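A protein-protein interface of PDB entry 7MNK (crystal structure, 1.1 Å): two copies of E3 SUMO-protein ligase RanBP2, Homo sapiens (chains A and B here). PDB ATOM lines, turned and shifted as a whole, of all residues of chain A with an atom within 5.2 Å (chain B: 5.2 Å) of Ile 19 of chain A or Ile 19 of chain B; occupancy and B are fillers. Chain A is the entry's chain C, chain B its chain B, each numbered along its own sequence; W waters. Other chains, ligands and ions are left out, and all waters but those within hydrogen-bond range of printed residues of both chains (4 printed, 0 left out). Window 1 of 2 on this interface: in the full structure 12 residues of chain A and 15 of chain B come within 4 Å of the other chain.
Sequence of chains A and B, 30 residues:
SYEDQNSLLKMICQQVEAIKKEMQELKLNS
Water W3 lies within hydrogen-bond range of the side-chain carboxylate of Glu 22 of chain A (2.7 Å) and the side-chain amide nitrogen of Gln 15 of chain B (2.9 Å).
Water W1 lies within hydrogen-bond range of O of Gln 15 of chain A (2.8 Å) and OE1 of Gln 15 of chain B (2.8 Å).
Water W2 bridges the side-chain amide oxygen (OE1) of Gln 15 of chain A and the backbone carbonyl oxygen (O) of Gln 15 of chain B.
Water W4 bridges the side-chain carboxylate of Glu 22 of chain B (3.2 Å) and the side-chain amide oxygen of Gln 15 of chain A (3.3 Å).
OE1 of Gln 15 of chain B sits close to OE1 of Glu 22 of chain A.
The side-chain carboxylate of Glu 22 of chain B is in hydrogen-bond range of the side-chain amide nitrogen of Gln 15 of chain A (2.7 Å).
Ile 12 of chain A touches Glu 22 of chain B.
Met 23 of chain B touches Ile 12 of chain A (SD to CG2, 3.97 Å).
CG1 of Ile 19 of chain B touches CB of Gln 15 of chain A (3.7 Å).
Gln 15 of chain B touches Ile 19 of chain A.
Ile 19 of chain A touches Val 16 of chain B.
CD1 of Ile 19 of chain A touches CD1 of Ile 19 of chain B (3.8 Å).
O of Glu 22 of chain A touches CD1 of Ile 12 of chain B, at 3.8 Å.
CE of Met 23 of chain A touches CG2 of Ile 12 of chain B (3.7 Å).
Ile 12 of chain A touches Glu 22 of chain B, and with the chains exchanged Glu 22 of chain A touches Ile 12 of chain B.
Ile 12 of chain A touches Met 23 of chain B, and with the chains exchanged Met 23 of chain A touches Ile 12 of chain B.
Gln 15 of chain A touches Ile 19 of chain B, and with the chains exchanged Ile 19 of chain A touches Gln 15 of chain B.
Ile 19 of chain A touches Val 16 of chain B, but with the chains exchanged Val 16 of chain A does not touch Ile 19 of chain B (4.02 Å).
11 positions are printed for both chains.
Printed residues of chain B within 4 Å of Ile 12 of chain A: Glu 22 (3.7 Å) and Met 23 (3.97 Å).
Of the printed residues of chain B, Gln 15 of chain A touches Ile 19 and Glu 22.
Ile 19 of chain A touches just these residues of chain B: Gln 15 (3.6 Å), Val 16 (3.95 Å) and Ile 19 (3.8 Å).
Of the printed residues of chain A, Gln 15 of chain B touches Ile 19 (3.6 Å) and Glu 22 (2.8 Å).
Of the printed residues of chain A, Val 16 of chain B touches Ile 19.
Of the printed residues of chain A, Ile 19 of chain B touches Gln 15 and Ile 19.
Of the printed residues of chain A, Met 23 of chain B touches Ile 12.
Gln 24 of chain B touches none of the printed residues of chain A.
The nearest printed residue of chain A that does not touch Ile 19 of chain B is Val 16 of chain A (4.02 Å).
Printed residues of chain B that touch a printed residue of chain A: Ile 12, Gln 15, Val 16, Ile 19, Glu 22 and Met 23.
Hydrophobic or aromatic side chains of chain B within 4 Å of the printed part of chain A: Ile 12, Val 16, Ile 19 and Met 23.
Among the printed residues, 10 pairs touch across the chains.
Among the printed residues, no Asp or Glu carboxylate lies within 4 Å of a Lys or Arg side-chain nitrogen of the other chain.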
ATOM      1  N   ILE A  12      -0.725 -11.846  12.121  1.00  0.00           N
ATOM      2  CA  ILE A  12       0.153 -12.325  13.179  1.00  0.00           C
ATOM      3  C   ILE A  12       0.879 -13.594  12.764  1.00  0.00           C
ATOM      4  O   ILE A  12       2.093 -13.728  12.980  1.00  0.00           O
ATOM      5  CB  ILE A  12      -0.636 -12.552  14.477  1.00  0.00           C
ATOM      6  CG1 ILE A  12      -1.186 -11.244  15.017  1.00  0.00           C
ATOM      7  CG2 ILE A  12       0.244 -13.247  15.496  1.00  0.00           C
ATOM      8  CD1 ILE A  12      -2.237 -11.402  16.112  1.00  0.00           C
ATOM      9  N   GLN A  15       3.663 -12.726  10.489  1.00  0.00           N
ATOM     10  CA  GLN A  15       4.731 -12.069  11.232  1.00  0.00           C
ATOM     11  C   GLN A  15       5.545 -13.055  12.058  1.00  0.00           C
ATOM     12  O   GLN A  15       6.766 -12.909  12.182  1.00  0.00           O
ATOM     13  CB  GLN A  15       4.160 -10.906  12.056  1.00  0.00           C
ATOM     14  CG  GLN A  15       3.720  -9.758  11.129  1.00  0.00           C
ATOM     15  CD  GLN A  15       2.908  -8.635  11.801  1.00  0.00           C
ATOM     16  OE1 GLN A  15       3.438  -7.858  12.621  1.00  0.00           O
ATOM     17  NE2 GLN A  15       1.637  -8.533  11.453  1.00  0.00           N
ATOM     18  N   VAL A  16       4.891 -14.075  12.615  1.00  0.00           N
ATOM     19  CA  VAL A  16       5.577 -15.105  13.389  1.00  0.00           C
ATOM     20  C   VAL A  16       6.501 -15.924  12.488  1.00  0.00           C
ATOM     21  O   VAL A  16       7.647 -16.225  12.851  1.00  0.00           O
ATOM     22  CB  VAL A  16       4.573 -15.998  14.139  1.00  0.00           C
ATOM     23  CG1 VAL A  16       5.239 -17.221  14.683  1.00  0.00           C
ATOM     24  CG2 VAL A  16       3.948 -15.218  15.292  1.00  0.00           C
ATOM     25  N   GLU A  17       6.019 -16.283  11.293  1.00  0.00           N
ATOM     26  CA  GLU A  17       6.887 -16.988  10.359  1.00  0.00           C
ATOM     27  C   GLU A  17       8.110 -16.145   9.976  1.00  0.00           C
ATOM     28  O   GLU A  17       9.203 -16.672   9.846  1.00  0.00           O
ATOM     29  CB  GLU A  17       6.104 -17.435   9.149  1.00  0.00           C
ATOM     30  CG  GLU A  17       6.920 -18.184   8.167  1.00  0.00           C
ATOM     31  CD  GLU A  17       7.470 -19.532   8.623  1.00  0.00           C
ATOM     32  OE1 GLU A  17       7.041 -20.078   9.640  1.00  0.00           O
ATOM     33  OE2 GLU A  17       8.368 -20.066   7.920  1.00  0.00           O
ATOM     34  N   ALA A  18       7.928 -14.843   9.751  1.00  0.00           N
ATOM     35  CA  ALA A  18       9.052 -13.962   9.425  1.00  0.00           C
ATOM     36  C   ALA A  18      10.084 -13.934  10.543  1.00  0.00           C
ATOM     37  O   ALA A  18      11.294 -14.002  10.274  1.00  0.00           O
ATOM     38  CB  ALA A  18       8.562 -12.555   9.096  1.00  0.00           C
ATOM     39  N   ILE A  19       9.647 -13.815  11.804  1.00  0.00           N
ATOM     40  CA  ILE A  19      10.618 -13.803  12.887  1.00  0.00           C
ATOM     41  C   ILE A  19      11.303 -15.153  13.009  1.00  0.00           C
ATOM     42  O   ILE A  19      12.504 -15.212  13.308  1.00  0.00           O
ATOM     43  CB  ILE A  19      10.090 -13.276  14.225  1.00  0.00           C
ATOM     44  CG1 ILE A  19       9.009 -14.091  14.854  1.00  0.00           C
ATOM     45  CG2 ILE A  19       9.771 -11.811  14.203  1.00  0.00           C
ATOM     46  CD1 ILE A  19       8.792 -13.783  16.343  1.00  0.00           C
ATOM     47  N   LYS A  20      10.582 -16.258  12.775  1.00  0.00           N
ATOM     48  CA  LYS A  20      11.223 -17.568  12.789  1.00  0.00           C
ATOM     49  C   LYS A  20      12.377 -17.608  11.792  1.00  0.00           C
ATOM     50  O   LYS A  20      13.480 -18.061  12.109  1.00  0.00           O
ATOM     51  CB  LYS A  20      10.192 -18.656  12.493  1.00  0.00           C
ATOM     52  CG  LYS A  20      10.786 -20.036  12.385  1.00  0.00           C
ATOM     53  CD  LYS A  20       9.786 -21.145  12.066  1.00  0.00           C
ATOM     54  CE  LYS A  20      10.468 -22.475  11.903  1.00  0.00           C
ATOM     55  NZ  LYS A  20       9.519 -23.548  11.512  1.00  0.00           N
ATOM     56  N   LYS A  21      12.120 -17.169  10.564  1.00  0.00           N
ATOM     57  CA  LYS A  21      13.156 -17.199   9.539  1.00  0.00           C
ATOM     58  C   LYS A  21      14.320 -16.284   9.880  1.00  0.00           C
ATOM     59  O   LYS A  21      15.467 -16.610   9.597  1.00  0.00           O
ATOM     60  CB  LYS A  21      12.542 -16.811   8.199  1.00  0.00           C
ATOM     61  CG  LYS A  21      11.606 -17.867   7.659  1.00  0.00           C
ATOM     62  CD  LYS A  21      11.141 -17.541   6.268  1.00  0.00           C
ATOM     63  CE  LYS A  21      10.349 -18.699   5.672  1.00  0.00           C
ATOM     64  NZ  LYS A  21       9.074 -18.263   5.040  1.00  0.00           N
ATOM     65  N   GLU A  22      14.041 -15.130  10.463  1.00  0.00           N
ATOM     66  CA  GLU A  22      15.090 -14.185  10.818  1.00  0.00           C
ATOM     67  C   GLU A  22      15.925 -14.673  11.996  1.00  0.00           C
ATOM     68  O   GLU A  22      17.147 -14.477  12.014  1.00  0.00           O
ATOM     69  CB  GLU A  22      14.483 -12.816  11.109  1.00  0.00           C
ATOM     70  CG  GLU A  22      13.964 -12.177   9.822  1.00  0.00           C
ATOM     71  CD  GLU A  22      12.749 -11.307   9.997  1.00  0.00           C
ATOM     72  OE1 GLU A  22      12.493 -10.854  11.159  1.00  0.00           O
ATOM     73  OE2 GLU A  22      11.991 -11.104   9.013  1.00  0.00           O
ATOM     74  N   MET A  23      15.302 -15.321  12.979  1.00  0.00           N
ATOM     75  CA  MET A  23      16.048 -15.917  14.088  1.00  0.00           C
ATOM     76  C   MET A  23      16.938 -17.041  13.595  1.00  0.00           C
ATOM     77  O   MET A  23      18.063 -17.204  14.083  1.00  0.00           O
ATOM     78  CB  MET A  23      15.065 -16.401  15.148  1.00  0.00           C
ATOM     79  CG  MET A  23      14.450 -15.261  15.906  1.00  0.00           C
ATOM     80  SD  MET A  23      13.053 -15.927  16.845  1.00  0.00           S
ATOM     81  CE  MET A  23      12.631 -14.453  17.748  1.00  0.00           C
ATOM     82  N   GLN A  24      16.456 -17.814  12.614  1.00  0.00           N
ATOM     83  CA  GLN A  24      17.304 -18.832  12.012  1.00  0.00           C
ATOM     84  C   GLN A  24      18.469 -18.195  11.270  1.00  0.00           C
ATOM     85  O   GLN A  24      19.607 -18.660  11.390  1.00  0.00           O
ATOM     86  CB  GLN A  24      16.473 -19.705  11.084  1.00  0.00           C
ATOM     87  CG  GLN A  24      15.542 -20.608  11.845  1.00  0.00           C
ATOM     88  CD  GLN A  24      14.738 -21.480  10.916  1.00  0.00           C
ATOM     89  OE1 GLN A  24      14.423 -21.090   9.774  1.00  0.00           O
ATOM     90  NE2 GLN A  24      14.394 -22.677  11.382  1.00  0.00           N
ATOM     91  N   ILE B  12      14.548  -7.986  14.574  1.00  0.00           N
ATOM     92  CA  ILE B  12      13.806  -9.017  15.284  1.00  0.00           C
ATOM     93  C   ILE B  12      13.105  -8.433  16.493  1.00  0.00           C
ATOM     94  O   ILE B  12      11.923  -8.705  16.741  1.00  0.00           O
ATOM     95  CB  ILE B  12      14.715 -10.208  15.667  1.00  0.00           C
ATOM     96  CG1 ILE B  12      15.210 -10.915  14.414  1.00  0.00           C
ATOM     97  CG2 ILE B  12      13.936 -11.181  16.543  1.00  0.00           C
ATOM     98  CD1 ILE B  12      16.407 -11.838  14.672  1.00  0.00           C
ATOM     99  N   GLN B  15      10.080  -6.479  15.462  1.00  0.00           N
ATOM    100  CA  GLN B  15       9.004  -7.325  14.988  1.00  0.00           C
ATOM    101  C   GLN B  15       8.338  -8.103  16.117  1.00  0.00           C
ATOM    102  O   GLN B  15       7.124  -8.313  16.085  1.00  0.00           O
ATOM    103  CB  GLN B  15       9.549  -8.215  13.881  1.00  0.00           C
ATOM    104  CG  GLN B  15       9.739  -7.388  12.618  1.00  0.00           C
ATOM    105  CD  GLN B  15      10.269  -8.126  11.415  1.00  0.00           C
ATOM    106  OE1 GLN B  15      10.133  -9.350  11.326  1.00  0.00           O
ATOM    107  NE2 GLN B  15      10.780  -7.400  10.473  1.00  0.00           N
ATOM    108  N   VAL B  16       9.098  -8.510  17.130  1.00  0.00           N
ATOM    109  CA  VAL B  16       8.514  -9.137  18.305  1.00  0.00           C
ATOM    110  C   VAL B  16       7.595  -8.172  19.043  1.00  0.00           C
ATOM    111  O   VAL B  16       6.482  -8.542  19.449  1.00  0.00           O
ATOM    112  CB  VAL B  16       9.586  -9.737  19.214  1.00  0.00           C
ATOM    113  CG1 VAL B  16       8.987 -10.194  20.537  1.00  0.00           C
ATOM    114  CG2 VAL B  16      10.321 -10.888  18.556  1.00  0.00           C
ATOM    115  N   GLU B  17       8.010  -6.917  19.199  1.00  0.00           N
ATOM    116  CA  GLU B  17       7.160  -5.926  19.844  1.00  0.00           C
ATOM    117  C   GLU B  17       5.887  -5.711  19.041  1.00  0.00           C
ATOM    118  O   GLU B  17       4.797  -5.573  19.621  1.00  0.00           O
ATOM    119  CB  GLU B  17       7.943  -4.621  20.035  1.00  0.00           C
ATOM    120  CG  GLU B  17       7.072  -3.471  20.563  1.00  0.00           C
ATOM    121  CD  GLU B  17       6.456  -3.693  21.918  1.00  0.00           C
ATOM    122  OE1 GLU B  17       6.861  -4.586  22.663  1.00  0.00           O
ATOM    123  OE2 GLU B  17       5.521  -2.914  22.244  1.00  0.00           O
ATOM    124  N   ALA B  18       5.987  -5.670  17.715  1.00  0.00           N
ATOM    125  CA  ALA B  18       4.782  -5.487  16.895  1.00  0.00           C
ATOM    126  C   ALA B  18       3.801  -6.644  17.089  1.00  0.00           C
ATOM    127  O   ALA B  18       2.583  -6.430  17.209  1.00  0.00           O
ATOM    128  CB  ALA B  18       5.162  -5.325  15.435  1.00  0.00           C
ATOM    129  N   ILE B  19       4.306  -7.885  17.141  1.00  0.00           N
ATOM    130  CA  ILE B  19       3.459  -9.041  17.396  1.00  0.00           C
ATOM    131  C   ILE B  19       2.833  -8.958  18.757  1.00  0.00           C
ATOM    132  O   ILE B  19       1.668  -9.296  18.922  1.00  0.00           O
ATOM    133  CB  ILE B  19       4.286 -10.333  17.205  1.00  0.00           C
ATOM    134  CG1 ILE B  19       4.669 -10.536  15.749  1.00  0.00           C
ATOM    135  CG2 ILE B  19       3.552 -11.542  17.776  1.00  0.00           C
ATOM    136  CD1 ILE B  19       5.857 -11.493  15.542  1.00  0.00           C
ATOM    137  N   LYS B  20       3.600  -8.556  19.776  1.00  0.00           N
ATOM    138  CA  LYS B  20       3.042  -8.371  21.114  1.00  0.00           C
ATOM    139  C   LYS B  20       1.823  -7.481  21.084  1.00  0.00           C
ATOM    140  O   LYS B  20       0.775  -7.809  21.662  1.00  0.00           O
ATOM    141  CB  LYS B  20       4.100  -7.818  22.081  1.00  0.00           C
ATOM    142  CG  LYS B  20       3.541  -7.475  23.457  1.00  0.00           C
ATOM    143  CD  LYS B  20       4.516  -6.824  24.407  1.00  0.00           C
ATOM    144  CE  LYS B  20       3.845  -6.463  25.734  1.00  0.00           C
ATOM    145  NZ  LYS B  20       4.787  -5.824  26.674  1.00  0.00           N
ATOM    146  N   LYS B  21       1.945  -6.332  20.442  1.00  0.00           N
ATOM    147  CA  LYS B  21       0.821  -5.403  20.415  1.00  0.00           C
ATOM    148  C   LYS B  21      -0.372  -6.010  19.696  1.00  0.00           C
ATOM    149  O   LYS B  21      -1.513  -5.846  20.137  1.00  0.00           O
ATOM    150  CB  LYS B  21       1.237  -4.075  19.761  1.00  0.00           C
ATOM    151  CG  LYS B  21       2.278  -3.301  20.548  1.00  0.00           C
ATOM    152  CD  LYS B  21       2.686  -2.013  19.838  1.00  0.00           C
ATOM    153  CE  LYS B  21       1.601  -0.936  19.953  1.00  0.00           C
ATOM    154  NZ  LYS B  21       1.495  -0.415  21.332  1.00  0.00           N
ATOM    155  N   GLU B  22      -0.139  -6.686  18.572  1.00  0.00           N
ATOM    156  CA  GLU B  22      -1.243  -7.312  17.852  1.00  0.00           C
ATOM    157  C   GLU B  22      -1.919  -8.396  18.682  1.00  0.00           C
ATOM    158  O   GLU B  22      -3.150  -8.526  18.677  1.00  0.00           O
ATOM    159  CB  GLU B  22      -0.743  -7.930  16.560  1.00  0.00           C
ATOM    160  CG  GLU B  22      -0.444  -6.936  15.493  1.00  0.00           C
ATOM    161  CD  GLU B  22       0.350  -7.572  14.406  1.00  0.00           C
ATOM    162  OE1 GLU B  22       1.431  -8.123  14.739  1.00  0.00           O
ATOM    163  OE2 GLU B  22      -0.069  -7.562  13.236  1.00  0.00           O
ATOM    164  N   MET B  23      -1.136  -9.204  19.376  1.00  0.00           N
ATOM    165  CA  MET B  23      -1.698 -10.265  20.205  1.00  0.00           C
ATOM    166  C   MET B  23      -2.611  -9.685  21.276  1.00  0.00           C
ATOM    167  O   MET B  23      -3.647 -10.256  21.590  1.00  0.00           O
ATOM    168  CB  MET B  23      -0.557 -11.074  20.832  1.00  0.00           C
ATOM    169  CG  MET B  23       0.128 -12.037  19.906  1.00  0.00           C
ATOM    170  SD  MET B  23      -0.849 -13.448  19.306  1.00  0.00           S
ATOM    171  CE  MET B  23      -1.627 -13.940  20.834  1.00  0.00           C
ATOM    172  N   GLN B  24      -2.236  -8.547  21.840  1.00  0.00           N
ATOM    173  CA  GLN B  24      -3.037  -7.867  22.844  1.00  0.00           C
ATOM    174  C   GLN B  24      -4.320  -7.309  22.258  1.00  0.00           C
ATOM    175  O   GLN B  24      -5.283  -7.088  22.985  1.00  0.00           O
ATOM    176  CB  GLN B  24      -2.234  -6.717  23.471  1.00  0.00           C
ATOM    177  CG  GLN B  24      -1.045  -7.127  24.283  1.00  0.00           C
ATOM    178  CD  GLN B  24      -0.215  -5.941  24.763  1.00  0.00           C
ATOM    179  OE1 GLN B  24      -0.180  -4.875  24.133  1.00  0.00           O
ATOM    180  NE2 GLN B  24       0.450  -6.126  25.887  1.00  0.00           N
HETATM  181  O   HOH W   1       7.497 -10.211  11.862  1.00  0.00           O
HETATM  182  O   HOH W   2       6.148  -8.249  13.283  1.00  0.00           O
HETATM  183  O   HOH W   3      11.190  -8.736   7.947  1.00  0.00           O
HETATM  184  O   HOH W   4       1.908  -5.061  13.468  1.00  0.00           O
